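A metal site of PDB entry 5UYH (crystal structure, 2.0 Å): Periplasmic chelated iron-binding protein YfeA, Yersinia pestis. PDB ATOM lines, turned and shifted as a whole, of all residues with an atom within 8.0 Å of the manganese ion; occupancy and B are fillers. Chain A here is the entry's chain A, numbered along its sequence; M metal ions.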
ATOM      1  N   GLU A  74     -17.753 -19.215  29.155  1.00  0.00           N
ATOM      2  CA  GLU A  74     -19.080 -18.884  28.660  1.00  0.00           C
ATOM      3  C   GLU A  74     -18.985 -17.643  27.760  1.00  0.00           C
ATOM      4  O   GLU A  74     -18.376 -16.641  28.140  1.00  0.00           O
ATOM      5  CB  GLU A  74     -20.016 -18.650  29.851  1.00  0.00           C
ATOM      6  CG  GLU A  74     -21.499 -18.894  29.584  1.00  0.00           C
ATOM      7  CD  GLU A  74     -22.098 -17.851  28.660  1.00  0.00           C
ATOM      8  OE1 GLU A  74     -22.065 -16.647  28.994  1.00  0.00           O
ATOM      9  OE2 GLU A  74     -22.608 -18.244  27.579  1.00  0.00           O
ATOM     10  N   ILE A  75     -19.555 -17.724  26.553  1.00  0.00           N
ATOM     11  CA  ILE A  75     -19.305 -16.689  25.536  1.00  0.00           C
ATOM     12  C   ILE A  75     -20.428 -15.659  25.402  1.00  0.00           C
ATOM     13  O   ILE A  75     -20.163 -14.540  24.938  1.00  0.00           O
ATOM     14  CB  ILE A  75     -19.028 -17.322  24.158  1.00  0.00           C
ATOM     15  CG1 ILE A  75     -20.288 -18.038  23.634  1.00  0.00           C
ATOM     16  CG2 ILE A  75     -17.831 -18.283  24.227  1.00  0.00           C
ATOM     17  CD1 ILE A  75     -20.051 -18.735  22.260  1.00  0.00           C
ATOM     18  N   HIS A  76     -21.670 -15.996  25.766  1.00  0.00           N
ATOM     19  CA  HIS A  76     -22.783 -15.074  25.528  1.00  0.00           C
ATOM     20  C   HIS A  76     -22.666 -13.832  26.409  1.00  0.00           C
ATOM     21  O   HIS A  76     -22.933 -12.715  25.957  1.00  0.00           O
ATOM     22  CB  HIS A  76     -24.141 -15.734  25.788  1.00  0.00           C
ATOM     23  CG  HIS A  76     -24.458 -16.898  24.900  1.00  0.00           C
ATOM     24  ND1 HIS A  76     -25.443 -16.848  23.937  1.00  0.00           N
ATOM     25  CD2 HIS A  76     -23.936 -18.143  24.837  1.00  0.00           C
ATOM     26  CE1 HIS A  76     -25.524 -18.015  23.325  1.00  0.00           C
ATOM     27  NE2 HIS A  76     -24.601 -18.822  23.846  1.00  0.00           N
ATOM     28  N   LEU A 101     -24.981 -13.108  19.384  1.00  0.00           N
ATOM     29  CA  LEU A 101     -24.371 -14.125  20.225  1.00  0.00           C
ATOM     30  C   LEU A 101     -23.603 -13.468  21.380  1.00  0.00           C
ATOM     31  O   LEU A 101     -23.831 -13.770  22.561  1.00  0.00           O
ATOM     32  CB  LEU A 101     -23.423 -15.002  19.398  1.00  0.00           C
ATOM     33  CG  LEU A 101     -22.527 -15.979  20.204  1.00  0.00           C
ATOM     34  CD1 LEU A 101     -23.373 -17.097  20.833  1.00  0.00           C
ATOM     35  CD2 LEU A 101     -21.400 -16.579  19.351  1.00  0.00           C
ATOM     36  N   ASN A 139     -31.619 -17.289  16.939  1.00  0.00           N
ATOM     37  CA  ASN A 139     -30.783 -18.300  17.608  1.00  0.00           C
ATOM     38  C   ASN A 139     -29.377 -18.171  17.034  1.00  0.00           C
ATOM     39  O   ASN A 139     -29.194 -18.373  15.819  1.00  0.00           O
ATOM     40  CB  ASN A 139     -31.337 -19.714  17.392  1.00  0.00           C
ATOM     41  CG  ASN A 139     -30.564 -20.770  18.158  1.00  0.00           C
ATOM     42  OD1 ASN A 139     -29.321 -20.719  18.268  1.00  0.00           O
ATOM     43  ND2 ASN A 139     -31.285 -21.761  18.691  1.00  0.00           N
ATOM     44  N   PRO A 140     -28.369 -17.821  17.830  1.00  0.00           N
ATOM     45  CA  PRO A 140     -27.068 -17.464  17.259  1.00  0.00           C
ATOM     46  C   PRO A 140     -26.173 -18.647  16.885  1.00  0.00           C
ATOM     47  O   PRO A 140     -25.139 -18.442  16.216  1.00  0.00           O
ATOM     48  CB  PRO A 140     -26.413 -16.638  18.373  1.00  0.00           C
ATOM     49  CG  PRO A 140     -26.986 -17.234  19.635  1.00  0.00           C
ATOM     50  CD  PRO A 140     -28.397 -17.678  19.308  1.00  0.00           C
ATOM     51  N   HIS A 141     -26.544 -19.882  17.240  1.00  0.00           N
ATOM     52  CA  HIS A 141     -25.626 -21.002  17.111  1.00  0.00           C
ATOM     53  C   HIS A 141     -25.622 -21.608  15.692  1.00  0.00           C
ATOM     54  O   HIS A 141     -25.753 -22.824  15.534  1.00  0.00           O
ATOM     55  CB  HIS A 141     -25.959 -22.097  18.143  1.00  0.00           C
ATOM     56  CG  HIS A 141     -26.050 -21.595  19.550  1.00  0.00           C
ATOM     57  ND1 HIS A 141     -27.225 -21.187  20.133  1.00  0.00           N
ATOM     58  CD2 HIS A 141     -25.100 -21.475  20.515  1.00  0.00           C
ATOM     59  CE1 HIS A 141     -27.009 -20.820  21.386  1.00  0.00           C
ATOM     60  NE2 HIS A 141     -25.723 -20.977  21.634  1.00  0.00           N
ATOM     61  N   TRP A 143     -23.314 -22.139  13.511  1.00  0.00           N
ATOM     62  CA  TRP A 143     -22.179 -22.962  13.112  1.00  0.00           C
ATOM     63  C   TRP A 143     -22.432 -24.449  13.356  1.00  0.00           C
ATOM     64  O   TRP A 143     -21.646 -25.271  12.885  1.00  0.00           O
ATOM     65  CB  TRP A 143     -20.901 -22.532  13.861  1.00  0.00           C
ATOM     66  CG  TRP A 143     -21.005 -22.684  15.349  1.00  0.00           C
ATOM     67  CD1 TRP A 143     -20.661 -23.785  16.088  1.00  0.00           C
ATOM     68  CD2 TRP A 143     -21.473 -21.694  16.281  1.00  0.00           C
ATOM     69  NE1 TRP A 143     -20.908 -23.537  17.431  1.00  0.00           N
ATOM     70  CE2 TRP A 143     -21.410 -22.278  17.576  1.00  0.00           C
ATOM     71  CE3 TRP A 143     -21.953 -20.392  16.154  1.00  0.00           C
ATOM     72  CZ2 TRP A 143     -21.799 -21.587  18.729  1.00  0.00           C
ATOM     73  CZ3 TRP A 143     -22.347 -19.705  17.299  1.00  0.00           C
ATOM     74  CH2 TRP A 143     -22.264 -20.297  18.574  1.00  0.00           C
ATOM     75  N   GLU A 207     -28.777 -25.937  27.215  1.00  0.00           N
ATOM     76  CA  GLU A 207     -29.066 -24.796  26.350  1.00  0.00           C
ATOM     77  C   GLU A 207     -29.696 -25.286  25.048  1.00  0.00           C
ATOM     78  O   GLU A 207     -29.336 -26.348  24.528  1.00  0.00           O
ATOM     79  CB  GLU A 207     -27.790 -23.979  26.051  1.00  0.00           C
ATOM     80  CG  GLU A 207     -28.086 -22.751  25.174  1.00  0.00           C
ATOM     81  CD  GLU A 207     -26.865 -21.898  24.789  1.00  0.00           C
ATOM     82  OE1 GLU A 207     -25.728 -22.422  24.610  1.00  0.00           O
ATOM     83  OE2 GLU A 207     -27.084 -20.671  24.632  1.00  0.00           O
ATOM     84  N   GLY A 208     -30.686 -24.538  24.558  1.00  0.00           N
ATOM     85  CA  GLY A 208     -31.265 -24.849  23.252  1.00  0.00           C
ATOM     86  C   GLY A 208     -30.360 -24.418  22.113  1.00  0.00           C
ATOM     87  O   GLY A 208     -30.757 -23.678  21.215  1.00  0.00           O
ATOM     88  N   ALA A 209     -29.128 -24.920  22.131  1.00  0.00           N
ATOM     89  CA  ALA A 209     -28.052 -24.470  21.259  1.00  0.00           C
ATOM     90  C   ALA A 209     -27.917 -25.299  19.982  1.00  0.00           C
ATOM     91  O   ALA A 209     -27.029 -25.017  19.175  1.00  0.00           O
ATOM     92  CB  ALA A 209     -26.734 -24.472  22.041  1.00  0.00           C
ATOM     93  N   PHE A 210     -28.758 -26.312  19.781  1.00  0.00           N
ATOM     94  CA  PHE A 210     -28.547 -27.271  18.711  1.00  0.00           C
ATOM     95  C   PHE A 210     -29.616 -27.209  17.628  1.00  0.00           C
ATOM     96  O   PHE A 210     -29.712 -28.141  16.813  1.00  0.00           O
ATOM     97  CB  PHE A 210     -28.416 -28.673  19.304  1.00  0.00           C
ATOM     98  CG  PHE A 210     -27.299 -28.782  20.292  1.00  0.00           C
ATOM     99  CD1 PHE A 210     -26.019 -29.117  19.876  1.00  0.00           C
ATOM    100  CD2 PHE A 210     -27.516 -28.480  21.630  1.00  0.00           C
ATOM    101  CE1 PHE A 210     -24.964 -29.171  20.787  1.00  0.00           C
ATOM    102  CE2 PHE A 210     -26.450 -28.524  22.543  1.00  0.00           C
ATOM    103  CZ  PHE A 210     -25.186 -28.872  22.117  1.00  0.00           C
ATOM    104  N   TRP A 225     -33.219 -24.453  28.890  1.00  0.00           N
ATOM    105  CA  TRP A 225     -33.388 -23.020  28.718  1.00  0.00           C
ATOM    106  C   TRP A 225     -33.049 -22.690  27.271  1.00  0.00           C
ATOM    107  O   TRP A 225     -32.135 -23.288  26.693  1.00  0.00           O
ATOM    108  CB  TRP A 225     -32.526 -22.165  29.660  1.00  0.00           C
ATOM    109  CG  TRP A 225     -31.040 -22.456  29.666  1.00  0.00           C
ATOM    110  CD1 TRP A 225     -30.081 -21.833  28.918  1.00  0.00           C
ATOM    111  CD2 TRP A 225     -30.352 -23.416  30.485  1.00  0.00           C
ATOM    112  NE1 TRP A 225     -28.831 -22.356  29.199  1.00  0.00           N
ATOM    113  CE2 TRP A 225     -28.978 -23.325  30.161  1.00  0.00           C
ATOM    114  CE3 TRP A 225     -30.766 -24.328  31.453  1.00  0.00           C
ATOM    115  CZ2 TRP A 225     -28.012 -24.125  30.779  1.00  0.00           C
ATOM    116  CZ3 TRP A 225     -29.812 -25.125  32.063  1.00  0.00           C
ATOM    117  CH2 TRP A 225     -28.454 -25.034  31.724  1.00  0.00           C
ATOM    118  N   PRO A 226     -33.749 -21.722  26.680  1.00  0.00           N
ATOM    119  CA  PRO A 226     -33.597 -21.503  25.232  1.00  0.00           C
ATOM    120  C   PRO A 226     -32.252 -20.927  24.818  1.00  0.00           C
ATOM    121  O   PRO A 226     -31.747 -21.279  23.749  1.00  0.00           O
ATOM    122  CB  PRO A 226     -34.764 -20.545  24.908  1.00  0.00           C
ATOM    123  CG  PRO A 226     -35.284 -20.057  26.235  1.00  0.00           C
ATOM    124  CD  PRO A 226     -34.946 -21.081  27.253  1.00  0.00           C
ATOM    125  N   ILE A 227     -31.647 -20.053  25.627  1.00  0.00           N
ATOM    126  CA  ILE A 227     -30.351 -19.470  25.288  1.00  0.00           C
ATOM    127  C   ILE A 227     -29.664 -19.076  26.591  1.00  0.00           C
ATOM    128  O   ILE A 227     -30.336 -18.708  27.562  1.00  0.00           O
ATOM    129  CB  ILE A 227     -30.506 -18.247  24.344  1.00  0.00           C
ATOM    130  CG1 ILE A 227     -29.145 -17.722  23.883  1.00  0.00           C
ATOM    131  CG2 ILE A 227     -31.308 -17.116  25.027  1.00  0.00           C
ATOM    132  CD1 ILE A 227     -29.210 -16.784  22.671  1.00  0.00           C
ATOM    133  N   ASN A 228     -28.328 -19.181  26.634  1.00  0.00           N
ATOM    134  CA  ASN A 228     -27.623 -18.836  27.861  1.00  0.00           C
ATOM    135  C   ASN A 228     -27.909 -17.395  28.231  1.00  0.00           C
ATOM    136  O   ASN A 228     -27.826 -16.487  27.385  1.00  0.00           O
ATOM    137  CB  ASN A 228     -26.098 -19.046  27.730  1.00  0.00           C
ATOM    138  CG  ASN A 228     -25.702 -20.520  27.637  1.00  0.00           C
ATOM    139  OD1 ASN A 228     -26.523 -21.424  27.786  1.00  0.00           O
ATOM    140  ND2 ASN A 228     -24.426 -20.758  27.353  1.00  0.00           N
ATOM    141  N   ALA A 229     -28.239 -17.178  29.514  1.00  0.00           N
ATOM    142  CA  ALA A 229     -28.531 -15.858  30.083  1.00  0.00           C
ATOM    143  C   ALA A 229     -28.877 -15.969  31.556  1.00  0.00           C
ATOM    144  O   ALA A 229     -29.320 -17.032  32.011  1.00  0.00           O
ATOM    145  CB  ALA A 229     -29.696 -15.175  29.349  1.00  0.00           C
ATOM    146  N   GLU A 256     -23.824 -29.291  28.190  1.00  0.00           N
ATOM    147  CA  GLU A 256     -22.846 -28.673  27.307  1.00  0.00           C
ATOM    148  C   GLU A 256     -21.648 -28.182  28.100  1.00  0.00           C
ATOM    149  O   GLU A 256     -21.720 -27.975  29.310  1.00  0.00           O
ATOM    150  CB  GLU A 256     -23.455 -27.524  26.502  1.00  0.00           C
ATOM    151  CG  GLU A 256     -24.601 -27.953  25.649  1.00  0.00           C
ATOM    152  CD  GLU A 256     -25.923 -27.802  26.391  1.00  0.00           C
ATOM    153  OE1 GLU A 256     -26.244 -26.659  26.774  1.00  0.00           O
ATOM    154  OE2 GLU A 256     -26.623 -28.815  26.609  1.00  0.00           O
ATOM    155  N   THR A 258     -19.694 -25.443  28.378  1.00  0.00           N
ATOM    156  CA  THR A 258     -19.419 -24.175  29.053  1.00  0.00           C
ATOM    157  C   THR A 258     -20.386 -23.873  30.192  1.00  0.00           C
ATOM    158  O   THR A 258     -20.249 -22.831  30.830  1.00  0.00           O
ATOM    159  CB  THR A 258     -19.416 -22.985  28.069  1.00  0.00           C
ATOM    160  OG1 THR A 258     -20.754 -22.707  27.631  1.00  0.00           O
ATOM    161  CG2 THR A 258     -18.476 -23.213  26.836  1.00  0.00           C
ATOM    162  N   ILE A 259     -21.355 -24.751  30.453  1.00  0.00           N
ATOM    163  CA  ILE A 259     -22.377 -24.493  31.482  1.00  0.00           C
ATOM    164  C   ILE A 259     -22.408 -25.655  32.482  1.00  0.00           C
ATOM    165  O   ILE A 259     -21.591 -26.572  32.403  1.00  0.00           O
ATOM    166  CB  ILE A 259     -23.760 -24.259  30.829  1.00  0.00           C
ATOM    167  CG1 ILE A 259     -24.060 -25.308  29.762  1.00  0.00           C
ATOM    168  CG2 ILE A 259     -23.836 -22.847  30.198  1.00  0.00           C
ATOM    169  CD1 ILE A 259     -24.758 -26.544  30.261  1.00  0.00           C
ATOM    170  N   VAL A 281     -20.565 -27.031  21.909  1.00  0.00           N
ATOM    171  CA  VAL A 281     -21.208 -26.118  20.960  1.00  0.00           C
ATOM    172  C   VAL A 281     -20.581 -24.729  21.057  1.00  0.00           C
ATOM    173  O   VAL A 281     -20.168 -24.164  20.043  1.00  0.00           O
ATOM    174  CB  VAL A 281     -22.740 -26.063  21.144  1.00  0.00           C
ATOM    175  CG1 VAL A 281     -23.138 -25.833  22.623  1.00  0.00           C
ATOM    176  CG2 VAL A 281     -23.366 -24.978  20.266  1.00  0.00           C
ATOM    177  N   ASP A 282     -20.508 -24.167  22.263  1.00  0.00           N
ATOM    178  CA  ASP A 282     -20.059 -22.789  22.395  1.00  0.00           C
ATOM    179  C   ASP A 282     -18.553 -22.654  22.537  1.00  0.00           C
ATOM    180  O   ASP A 282     -18.049 -21.529  22.544  1.00  0.00           O
ATOM    181  CB  ASP A 282     -20.687 -22.097  23.600  1.00  0.00           C
ATOM    182  CG  ASP A 282     -22.149 -21.804  23.403  1.00  0.00           C
ATOM    183  OD1 ASP A 282     -22.680 -21.934  22.272  1.00  0.00           O
ATOM    184  OD2 ASP A 282     -22.767 -21.430  24.416  1.00  0.00           O
ATOM    185  N   SER A 283     -17.818 -23.758  22.658  1.00  0.00           N
ATOM    186  CA  SER A 283     -16.370 -23.648  22.821  1.00  0.00           C
ATOM    187  C   SER A 283     -15.707 -24.925  22.352  1.00  0.00           C
ATOM    188  O   SER A 283     -16.281 -26.007  22.415  1.00  0.00           O
ATOM    189  CB  SER A 283     -15.965 -23.376  24.272  1.00  0.00           C
ATOM    190  OG  SER A 283     -14.547 -23.317  24.376  1.00  0.00           O
HETATM  191 MN    MN M   1     -24.738 -20.893  23.561  1.00  0.00          MN
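The backbone NH (N) of His 76 sits at hydrogen-bond distance from the side-chain carboxylate (OE2) of Glu 74, 3.0 Å away.
The backbone NH (N) of Asn 228 lies close to the side-chain carboxylate (OE2) of Glu 207 (2.8 Å).
The side-chain carboxylate (OE1) of Glu 256 is in hydrogen-bond range of the backbone NH (N) of Glu 207, 2.7 Å away.
A ring nitrogen (ND1) of His 141 is in hydrogen-bond range of the side-chain amide oxygen (OD1) of Asn 139 (2.8 Å).
The side-chain amide nitrogen (ND2) of Asn 228 lies close to the side-chain carboxylate (OD2) of Asp 282, at 3.4 Å.
The side-chain amide nitrogen of Asn 228 is in hydrogen-bond range of the side-chain carboxylate of Glu 74, at 3.1 Å.
OD1 of Asn 228 is in hydrogen-bond range of NE1 of Trp 225, at 2.9 Å.
The manganese ion is bound by a ring nitrogen (NE2) of His 76 (2.1 Å), the side-chain carboxylate (OE1) of Glu 207 (2.1 Å), a ring nitrogen (NE2) of His 141 (2.2 Å), the side-chain carboxylate (OD2) of Asp 282 (2.2 Å), the side-chain carboxylate (OE2) of Glu 207 (2.6 Å) and the side-chain carboxylate (OD1) of Asp 282 (2.6 Å).
Merely in contact with the manganese ion: Asn 228.
Five residues have an atom within 4 Å of the manganese ion: His 76, His 141, Glu 207, Asn 228 and Asp 282.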
